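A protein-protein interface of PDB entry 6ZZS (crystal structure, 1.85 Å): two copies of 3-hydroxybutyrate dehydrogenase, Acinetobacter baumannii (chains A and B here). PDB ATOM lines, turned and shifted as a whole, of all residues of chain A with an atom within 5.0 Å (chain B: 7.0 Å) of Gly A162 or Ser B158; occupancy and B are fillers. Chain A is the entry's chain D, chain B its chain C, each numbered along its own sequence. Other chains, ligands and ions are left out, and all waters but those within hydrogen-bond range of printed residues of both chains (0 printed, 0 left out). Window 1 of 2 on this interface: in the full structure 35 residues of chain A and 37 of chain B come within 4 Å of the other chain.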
ATOM      1  N   LEU A 116      26.364 -25.600 -18.537  1.00  0.00           N
ATOM      2  CA  LEU A 116      24.908 -25.653 -18.809  1.00  0.00           C
ATOM      3  C   LEU A 116      24.678 -25.707 -20.316  1.00  0.00           C
ATOM      4  O   LEU A 116      24.170 -26.761 -20.820  1.00  0.00           O
ATOM      5  CB  LEU A 116      24.211 -24.435 -18.202  1.00  0.00           C
ATOM      6  CG  LEU A 116      22.726 -24.342 -18.519  1.00  0.00           C
ATOM      7  CD1 LEU A 116      22.041 -25.636 -18.134  1.00  0.00           C
ATOM      8  CD2 LEU A 116      22.085 -23.182 -17.799  1.00  0.00           C
ATOM      9  N   ASN A 157      27.573 -23.007  -9.030  1.00  0.00           N
ATOM     10  CA  ASN A 157      26.343 -23.525  -8.377  1.00  0.00           C
ATOM     11  C   ASN A 157      25.155 -23.122  -9.261  1.00  0.00           C
ATOM     12  O   ASN A 157      24.178 -23.897  -9.325  1.00  0.00           O
ATOM     13  CB  ASN A 157      26.185 -23.048  -6.927  1.00  0.00           C
ATOM     14  CG  ASN A 157      27.070 -23.797  -5.954  1.00  0.00           C
ATOM     15  OD1 ASN A 157      28.229 -24.098  -6.243  1.00  0.00           O
ATOM     16  ND2 ASN A 157      26.526 -24.173  -4.819  1.00  0.00           N
ATOM     17  N   SER A 158      25.256 -21.993  -9.970  1.00  0.00           N
ATOM     18  CA  SER A 158      24.171 -21.541 -10.893  1.00  0.00           C
ATOM     19  C   SER A 158      24.130 -22.454 -12.127  1.00  0.00           C
ATOM     20  O   SER A 158      23.043 -22.869 -12.514  1.00  0.00           O
ATOM     21  CB  SER A 158      24.315 -20.112 -11.269  1.00  0.00           C
ATOM     22  OG  SER A 158      24.022 -19.269 -10.163  1.00  0.00           O
ATOM     23  N   ALA A 159      25.289 -22.820 -12.680  1.00  0.00           N
ATOM     24  CA  ALA A 159      25.371 -23.679 -13.886  1.00  0.00           C
ATOM     25  C   ALA A 159      24.882 -25.086 -13.527  1.00  0.00           C
ATOM     26  O   ALA A 159      24.080 -25.623 -14.298  1.00  0.00           O
ATOM     27  CB  ALA A 159      26.772 -23.700 -14.442  1.00  0.00           C
ATOM     28  N   LYS A 160      25.367 -25.640 -12.407  1.00  0.00           N
ATOM     29  CA  LYS A 160      25.062 -27.016 -11.943  1.00  0.00           C
ATOM     30  C   LYS A 160      23.574 -27.111 -11.533  1.00  0.00           C
ATOM     31  O   LYS A 160      22.934 -28.135 -11.877  1.00  0.00           O
ATOM     32  CB  LYS A 160      26.031 -27.433 -10.834  1.00  0.00           C
ATOM     33  CG  LYS A 160      27.506 -27.463 -11.215  1.00  0.00           C
ATOM     34  CD  LYS A 160      27.851 -28.348 -12.361  1.00  0.00           C
ATOM     35  CE  LYS A 160      29.301 -28.789 -12.305  1.00  0.00           C
ATOM     36  NZ  LYS A 160      29.618 -29.636 -13.466  1.00  0.00           N
ATOM     37  N   HIS A 161      23.005 -26.106 -10.857  1.00  0.00           N
ATOM     38  CA  HIS A 161      21.539 -26.062 -10.615  1.00  0.00           C
ATOM     39  C   HIS A 161      20.847 -26.145 -11.971  1.00  0.00           C
ATOM     40  O   HIS A 161      19.893 -26.952 -12.121  1.00  0.00           O
ATOM     41  CB  HIS A 161      21.083 -24.843  -9.782  1.00  0.00           C
ATOM     42  CG  HIS A 161      21.143 -25.087  -8.301  1.00  0.00           C
ATOM     43  ND1 HIS A 161      22.346 -25.168  -7.600  1.00  0.00           N
ATOM     44  CD2 HIS A 161      20.163 -25.297  -7.390  1.00  0.00           C
ATOM     45  CE1 HIS A 161      22.088 -25.416  -6.324  1.00  0.00           C
ATOM     46  NE2 HIS A 161      20.754 -25.455  -6.166  1.00  0.00           N
ATOM     47  N   GLY A 162      21.302 -25.340 -12.925  1.00  0.00           N
ATOM     48  CA  GLY A 162      20.622 -25.230 -14.220  1.00  0.00           C
ATOM     49  C   GLY A 162      20.693 -26.543 -14.958  1.00  0.00           C
ATOM     50  O   GLY A 162      19.665 -26.945 -15.469  1.00  0.00           O
ATOM     51  N   VAL A 163      21.838 -27.237 -14.930  1.00  0.00           N
ATOM     52  CA  VAL A 163      21.993 -28.547 -15.644  1.00  0.00           C
ATOM     53  C   VAL A 163      21.036 -29.605 -15.047  1.00  0.00           C
ATOM     54  O   VAL A 163      20.591 -30.494 -15.801  1.00  0.00           O
ATOM     55  CB  VAL A 163      23.461 -29.030 -15.719  1.00  0.00           C
ATOM     56  CG1 VAL A 163      23.819 -30.077 -14.681  1.00  0.00           C
ATOM     57  CG2 VAL A 163      23.773 -29.597 -17.089  1.00  0.00           C
ATOM     58  N   ILE A 164      20.673 -29.515 -13.770  1.00  0.00           N
ATOM     59  CA  ILE A 164      19.659 -30.427 -13.152  1.00  0.00           C
ATOM     60  C   ILE A 164      18.263 -30.068 -13.685  1.00  0.00           C
ATOM     61  O   ILE A 164      17.511 -31.004 -14.042  1.00  0.00           O
ATOM     62  CB  ILE A 164      19.769 -30.424 -11.618  1.00  0.00           C
ATOM     63  CG1 ILE A 164      21.070 -31.103 -11.178  1.00  0.00           C
ATOM     64  CG2 ILE A 164      18.562 -31.096 -10.972  1.00  0.00           C
ATOM     65  CD1 ILE A 164      21.405 -30.875  -9.733  1.00  0.00           C
ATOM     66  N   GLY A 165      17.947 -28.778 -13.815  1.00  0.00           N
ATOM     67  CA  GLY A 165      16.772 -28.298 -14.587  1.00  0.00           C
ATOM     68  C   GLY A 165      16.722 -28.875 -15.996  1.00  0.00           C
ATOM     69  O   GLY A 165      15.663 -29.356 -16.426  1.00  0.00           O
ATOM     70  N   LEU A 166      17.845 -28.837 -16.703  1.00  0.00           N
ATOM     71  CA  LEU A 166      17.928 -29.310 -18.106  1.00  0.00           C
ATOM     72  C   LEU A 166      17.755 -30.833 -18.129  1.00  0.00           C
ATOM     73  O   LEU A 166      17.085 -31.324 -19.057  1.00  0.00           O
ATOM     74  CB  LEU A 166      19.258 -28.865 -18.736  1.00  0.00           C
ATOM     75  CG  LEU A 166      19.570 -29.477 -20.101  1.00  0.00           C
ATOM     76  CD1 LEU A 166      18.591 -28.989 -21.147  1.00  0.00           C
ATOM     77  CD2 LEU A 166      20.989 -29.170 -20.527  1.00  0.00           C
ATOM     78  N   PHE B 108      17.780 -20.363 -25.990  1.00  0.00           N
ATOM     79  CA  PHE B 108      18.183 -21.033 -24.730  1.00  0.00           C
ATOM     80  C   PHE B 108      19.118 -20.081 -23.961  1.00  0.00           C
ATOM     81  O   PHE B 108      18.872 -19.815 -22.764  1.00  0.00           O
ATOM     82  CB  PHE B 108      18.856 -22.377 -25.039  1.00  0.00           C
ATOM     83  CG  PHE B 108      19.325 -23.113 -23.812  1.00  0.00           C
ATOM     84  CD1 PHE B 108      20.569 -22.840 -23.265  1.00  0.00           C
ATOM     85  CD2 PHE B 108      18.501 -24.037 -23.182  1.00  0.00           C
ATOM     86  CE1 PHE B 108      21.007 -23.523 -22.146  1.00  0.00           C
ATOM     87  CE2 PHE B 108      18.928 -24.683 -22.037  1.00  0.00           C
ATOM     88  CZ  PHE B 108      20.182 -24.427 -21.516  1.00  0.00           C
ATOM     89  N   VAL B 112      18.467 -17.772 -20.333  1.00  0.00           N
ATOM     90  CA  VAL B 112      19.439 -17.905 -19.210  1.00  0.00           C
ATOM     91  C   VAL B 112      20.069 -16.540 -18.896  1.00  0.00           C
ATOM     92  O   VAL B 112      20.231 -16.262 -17.701  1.00  0.00           O
ATOM     93  CB  VAL B 112      20.504 -18.968 -19.534  1.00  0.00           C
ATOM     94  CG1 VAL B 112      21.734 -18.825 -18.658  1.00  0.00           C
ATOM     95  CG2 VAL B 112      19.913 -20.365 -19.444  1.00  0.00           C
ATOM     96  N   LEU B 116      18.717 -15.716 -15.371  1.00  0.00           N
ATOM     97  CA  LEU B 116      19.819 -16.081 -14.444  1.00  0.00           C
ATOM     98  C   LEU B 116      20.837 -14.938 -14.387  1.00  0.00           C
ATOM     99  O   LEU B 116      21.037 -14.404 -13.280  1.00  0.00           O
ATOM    100  CB  LEU B 116      20.474 -17.386 -14.904  1.00  0.00           C
ATOM    101  CG  LEU B 116      21.679 -17.817 -14.089  1.00  0.00           C
ATOM    102  CD1 LEU B 116      21.291 -17.905 -12.618  1.00  0.00           C
ATOM    103  CD2 LEU B 116      22.241 -19.140 -14.609  1.00  0.00           C
ATOM    104  N   ASN B 145       9.060 -24.407 -11.997  1.00  0.00           N
ATOM    105  CA  ASN B 145       9.981 -24.861 -13.078  1.00  0.00           C
ATOM    106  C   ASN B 145      11.443 -24.642 -12.664  1.00  0.00           C
ATOM    107  O   ASN B 145      12.328 -25.146 -13.398  1.00  0.00           O
ATOM    108  CB  ASN B 145       9.625 -24.240 -14.434  1.00  0.00           C
ATOM    109  CG  ASN B 145       8.360 -24.836 -15.030  1.00  0.00           C
ATOM    110  OD1 ASN B 145       8.267 -26.046 -15.258  1.00  0.00           O
ATOM    111  ND2 ASN B 145       7.356 -24.011 -15.262  1.00  0.00           N
ATOM    112  N   GLY B 146      11.698 -23.982 -11.523  1.00  0.00           N
ATOM    113  CA  GLY B 146      12.994 -24.024 -10.826  1.00  0.00           C
ATOM    114  C   GLY B 146      13.229 -25.311 -10.052  1.00  0.00           C
ATOM    115  O   GLY B 146      14.412 -25.594  -9.699  1.00  0.00           O
ATOM    116  N   LYS B 153      10.483 -26.801 -22.179  1.00  0.00           N
ATOM    117  CA  LYS B 153      10.943 -25.580 -21.458  1.00  0.00           C
ATOM    118  C   LYS B 153      12.411 -25.715 -21.075  1.00  0.00           C
ATOM    119  O   LYS B 153      12.774 -25.218 -20.016  1.00  0.00           O
ATOM    120  CB  LYS B 153      10.045 -25.305 -20.255  1.00  0.00           C
ATOM    121  CG  LYS B 153       8.706 -24.684 -20.623  1.00  0.00           C
ATOM    122  CD  LYS B 153       7.678 -24.617 -19.525  1.00  0.00           C
ATOM    123  CE  LYS B 153       6.436 -23.873 -19.979  1.00  0.00           C
ATOM    124  NZ  LYS B 153       5.225 -24.205 -19.198  1.00  0.00           N
ATOM    125  N   ALA B 154      13.240 -26.322 -21.922  1.00  0.00           N
ATOM    126  CA  ALA B 154      14.668 -26.524 -21.595  1.00  0.00           C
ATOM    127  C   ALA B 154      15.285 -25.203 -21.076  1.00  0.00           C
ATOM    128  O   ALA B 154      16.006 -25.199 -20.047  1.00  0.00           O
ATOM    129  CB  ALA B 154      15.385 -27.038 -22.804  1.00  0.00           C
ATOM    130  N   GLY B 155      15.031 -24.104 -21.785  1.00  0.00           N
ATOM    131  CA  GLY B 155      15.663 -22.802 -21.522  1.00  0.00           C
ATOM    132  C   GLY B 155      15.144 -22.219 -20.236  1.00  0.00           C
ATOM    133  O   GLY B 155      15.942 -21.832 -19.370  1.00  0.00           O
ATOM    134  N   TYR B 156      13.834 -22.167 -20.111  1.00  0.00           N
ATOM    135  CA  TYR B 156      13.170 -21.560 -18.941  1.00  0.00           C
ATOM    136  C   TYR B 156      13.488 -22.383 -17.681  1.00  0.00           C
ATOM    137  O   TYR B 156      13.850 -21.801 -16.640  1.00  0.00           O
ATOM    138  CB  TYR B 156      11.682 -21.439 -19.230  1.00  0.00           C
ATOM    139  CG  TYR B 156      10.892 -20.754 -18.158  1.00  0.00           C
ATOM    140  CD1 TYR B 156      10.352 -21.483 -17.105  1.00  0.00           C
ATOM    141  CD2 TYR B 156      10.666 -19.386 -18.198  1.00  0.00           C
ATOM    142  CE1 TYR B 156       9.600 -20.875 -16.122  1.00  0.00           C
ATOM    143  CE2 TYR B 156       9.914 -18.760 -17.221  1.00  0.00           C
ATOM    144  CZ  TYR B 156       9.361 -19.511 -16.194  1.00  0.00           C
ATOM    145  OH  TYR B 156       8.633 -18.900 -15.213  1.00  0.00           O
ATOM    146  N   ASN B 157      13.378 -23.703 -17.756  1.00  0.00           N
ATOM    147  CA  ASN B 157      13.566 -24.546 -16.547  1.00  0.00           C
ATOM    148  C   ASN B 157      15.044 -24.498 -16.153  1.00  0.00           C
ATOM    149  O   ASN B 157      15.310 -24.582 -14.958  1.00  0.00           O
ATOM    150  CB  ASN B 157      13.061 -25.981 -16.712  1.00  0.00           C
ATOM    151  CG  ASN B 157      11.560 -26.068 -16.542  1.00  0.00           C
ATOM    152  OD1 ASN B 157      10.809 -25.256 -17.088  1.00  0.00           O
ATOM    153  ND2 ASN B 157      11.103 -27.024 -15.766  1.00  0.00           N
ATOM    154  N   SER B 158      15.956 -24.401 -17.120  1.00  0.00           N
ATOM    155  CA  SER B 158      17.414 -24.329 -16.849  1.00  0.00           C
ATOM    156  C   SER B 158      17.720 -22.994 -16.167  1.00  0.00           C
ATOM    157  O   SER B 158      18.468 -22.980 -15.208  1.00  0.00           O
ATOM    158  CB  SER B 158      18.228 -24.528 -18.089  1.00  0.00           C
ATOM    159  OG  SER B 158      18.069 -25.847 -18.605  1.00  0.00           O
ATOM    160  N   ALA B 159      17.121 -21.912 -16.643  1.00  0.00           N
ATOM    161  CA  ALA B 159      17.333 -20.559 -16.099  1.00  0.00           C
ATOM    162  C   ALA B 159      16.821 -20.522 -14.660  1.00  0.00           C
ATOM    163  O   ALA B 159      17.583 -20.077 -13.788  1.00  0.00           O
ATOM    164  CB  ALA B 159      16.648 -19.530 -16.956  1.00  0.00           C
ATOM    165  N   LYS B 160      15.571 -20.942 -14.453  1.00  0.00           N
ATOM    166  CA  LYS B 160      14.889 -20.934 -13.134  1.00  0.00           C
ATOM    167  C   LYS B 160      15.600 -21.853 -12.130  1.00  0.00           C
ATOM    168  O   LYS B 160      15.774 -21.419 -10.970  1.00  0.00           O
ATOM    169  CB  LYS B 160      13.408 -21.269 -13.300  1.00  0.00           C
ATOM    170  CG  LYS B 160      12.622 -20.240 -14.090  1.00  0.00           C
ATOM    171  CD  LYS B 160      12.841 -18.812 -13.686  1.00  0.00           C
ATOM    172  CE  LYS B 160      11.727 -17.928 -14.208  1.00  0.00           C
ATOM    173  NZ  LYS B 160      11.752 -16.577 -13.606  1.00  0.00           N
ATOM    174  N   HIS B 161      16.011 -23.063 -12.529  1.00  0.00           N
ATOM    175  CA  HIS B 161      16.844 -23.942 -11.665  1.00  0.00           C
ATOM    176  C   HIS B 161      18.091 -23.161 -11.260  1.00  0.00           C
ATOM    177  O   HIS B 161      18.416 -23.145 -10.081  1.00  0.00           O
ATOM    178  CB  HIS B 161      17.232 -25.263 -12.335  1.00  0.00           C
ATOM    179  CG  HIS B 161      16.222 -26.336 -12.136  1.00  0.00           C
ATOM    180  ND1 HIS B 161      14.993 -26.322 -12.777  1.00  0.00           N
ATOM    181  CD2 HIS B 161      16.234 -27.421 -11.338  1.00  0.00           C
ATOM    182  CE1 HIS B 161      14.298 -27.370 -12.380  1.00  0.00           C
ATOM    183  NE2 HIS B 161      15.046 -28.062 -11.509  1.00  0.00           N
ATOM    184  N   GLY B 162      18.761 -22.530 -12.223  1.00  0.00           N
ATOM    185  CA  GLY B 162      20.011 -21.791 -11.973  1.00  0.00           C
ATOM    186  C   GLY B 162      19.818 -20.643 -11.011  1.00  0.00           C
ATOM    187  O   GLY B 162      20.678 -20.466 -10.121  1.00  0.00           O
ATOM    188  N   VAL B 163      18.720 -19.907 -11.112  1.00  0.00           N
ATOM    189  CA  VAL B 163      18.484 -18.727 -10.233  1.00  0.00           C
ATOM    190  C   VAL B 163      18.211 -19.191  -8.796  1.00  0.00           C
ATOM    191  O   VAL B 163      18.507 -18.415  -7.861  1.00  0.00           O
ATOM    192  CB  VAL B 163      17.375 -17.793 -10.770  1.00  0.00           C
ATOM    193  CG1 VAL B 163      15.984 -18.158 -10.327  1.00  0.00           C
ATOM    194  CG2 VAL B 163      17.629 -16.345 -10.375  1.00  0.00           C
ATOM    195  N   GLY B 165      19.890 -21.797  -7.563  1.00  0.00           N
ATOM    196  CA  GLY B 165      21.309 -21.991  -7.205  1.00  0.00           C
ATOM    197  C   GLY B 165      21.947 -20.662  -6.808  1.00  0.00           C
ATOM    198  O   GLY B 165      22.574 -20.607  -5.770  1.00  0.00           O
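A ring nitrogen (ND1) of His B161 lies within hydrogen-bond range of the backbone carbonyl oxygen (O) of Asn B157 (2.8 Å). The backbone carbonyl oxygen (O) of Asn B145 is in hydrogen-bond range of a ring nitrogen (ND1) of His B161 (3.0 Å). The backbone carbonyl oxygen (O) of Asn A157 sits at hydrogen-bond distance from a ring nitrogen (ND1) of His A161, 2.8 Å away. The backbone carbonyl oxygen of Ala B154 sits at hydrogen-bond distance from the side-chain hydroxyl of Ser B158 (2.6 Å). A ring nitrogen (NE2) of His B161 lies close to the backbone carbonyl oxygen (O) of Gly B146 (3.1 Å).
Among the printed residues, merely in contact across the chains: Leu A116 with Phe B108 (3.9 Å), Leu A116 with Val B112 (3.9 Å), Leu A116 with Ser B158 (3.97 Å), Ser A158 with Leu B116 (3.9 Å), Ser A158 with Gly B162 (3.3 Å), His A161 with His B161 (3.2 Å), His A161 with Gly B162 (3.9 Å), His A161 with Gly B165 (3.3 Å), Gly A162 with Ser B158 (3.3 Å), Gly A162 with His B161 (3.9 Å), Gly A162 with Gly B162 (3.8 Å), Gly A165 with His B161 (3.2 Å) and Leu A166 with Ser B158 (3.2 Å).
Of the printed residues of chain B, Leu A116 touches Phe B108, Val B112 and Ser B158. Ala A159 touches none of the printed residues of chain B. Printed residues of chain B within 4 Å of His A161: His B161 (3.2 Å), Gly B162 (3.9 Å) and Gly B165 (3.3 Å). Printed residues of chain B within 4 Å of Gly A162: Ser B158, His B161 and Gly B162. Ser B158 touches just these residues of chain A: Leu A116 (3.97 Å), Gly A162 (3.3 Å) and Leu A166 (3.2 Å). Val B163 touches none of the printed residues of chain A.
Of the 11 printed residues of chain A, 6 touch a printed residue of chain B. Hydrophobic or aromatic side chains of chain B within 4 Å of the printed part of chain A: Phe B108, Val B112, Leu B116 and His B161.
Leu A116 touches Ser B158, and with the chains exchanged Ser A158 touches Leu B116. His A161 touches Gly B162, and with the chains exchanged Gly A162 touches His B161. His A161 touches Gly B165, and with the chains exchanged Gly A165 touches His B161. Gly B162 touches its own counterpart, Gly A162. Positions printed for both chains: 116, 157, 158, 159, 160, 161, 162, 163 and 165. Of the 13 pairs that touch across the chains among the printed residues, 10 have their exchanged pair printed and touching as well.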
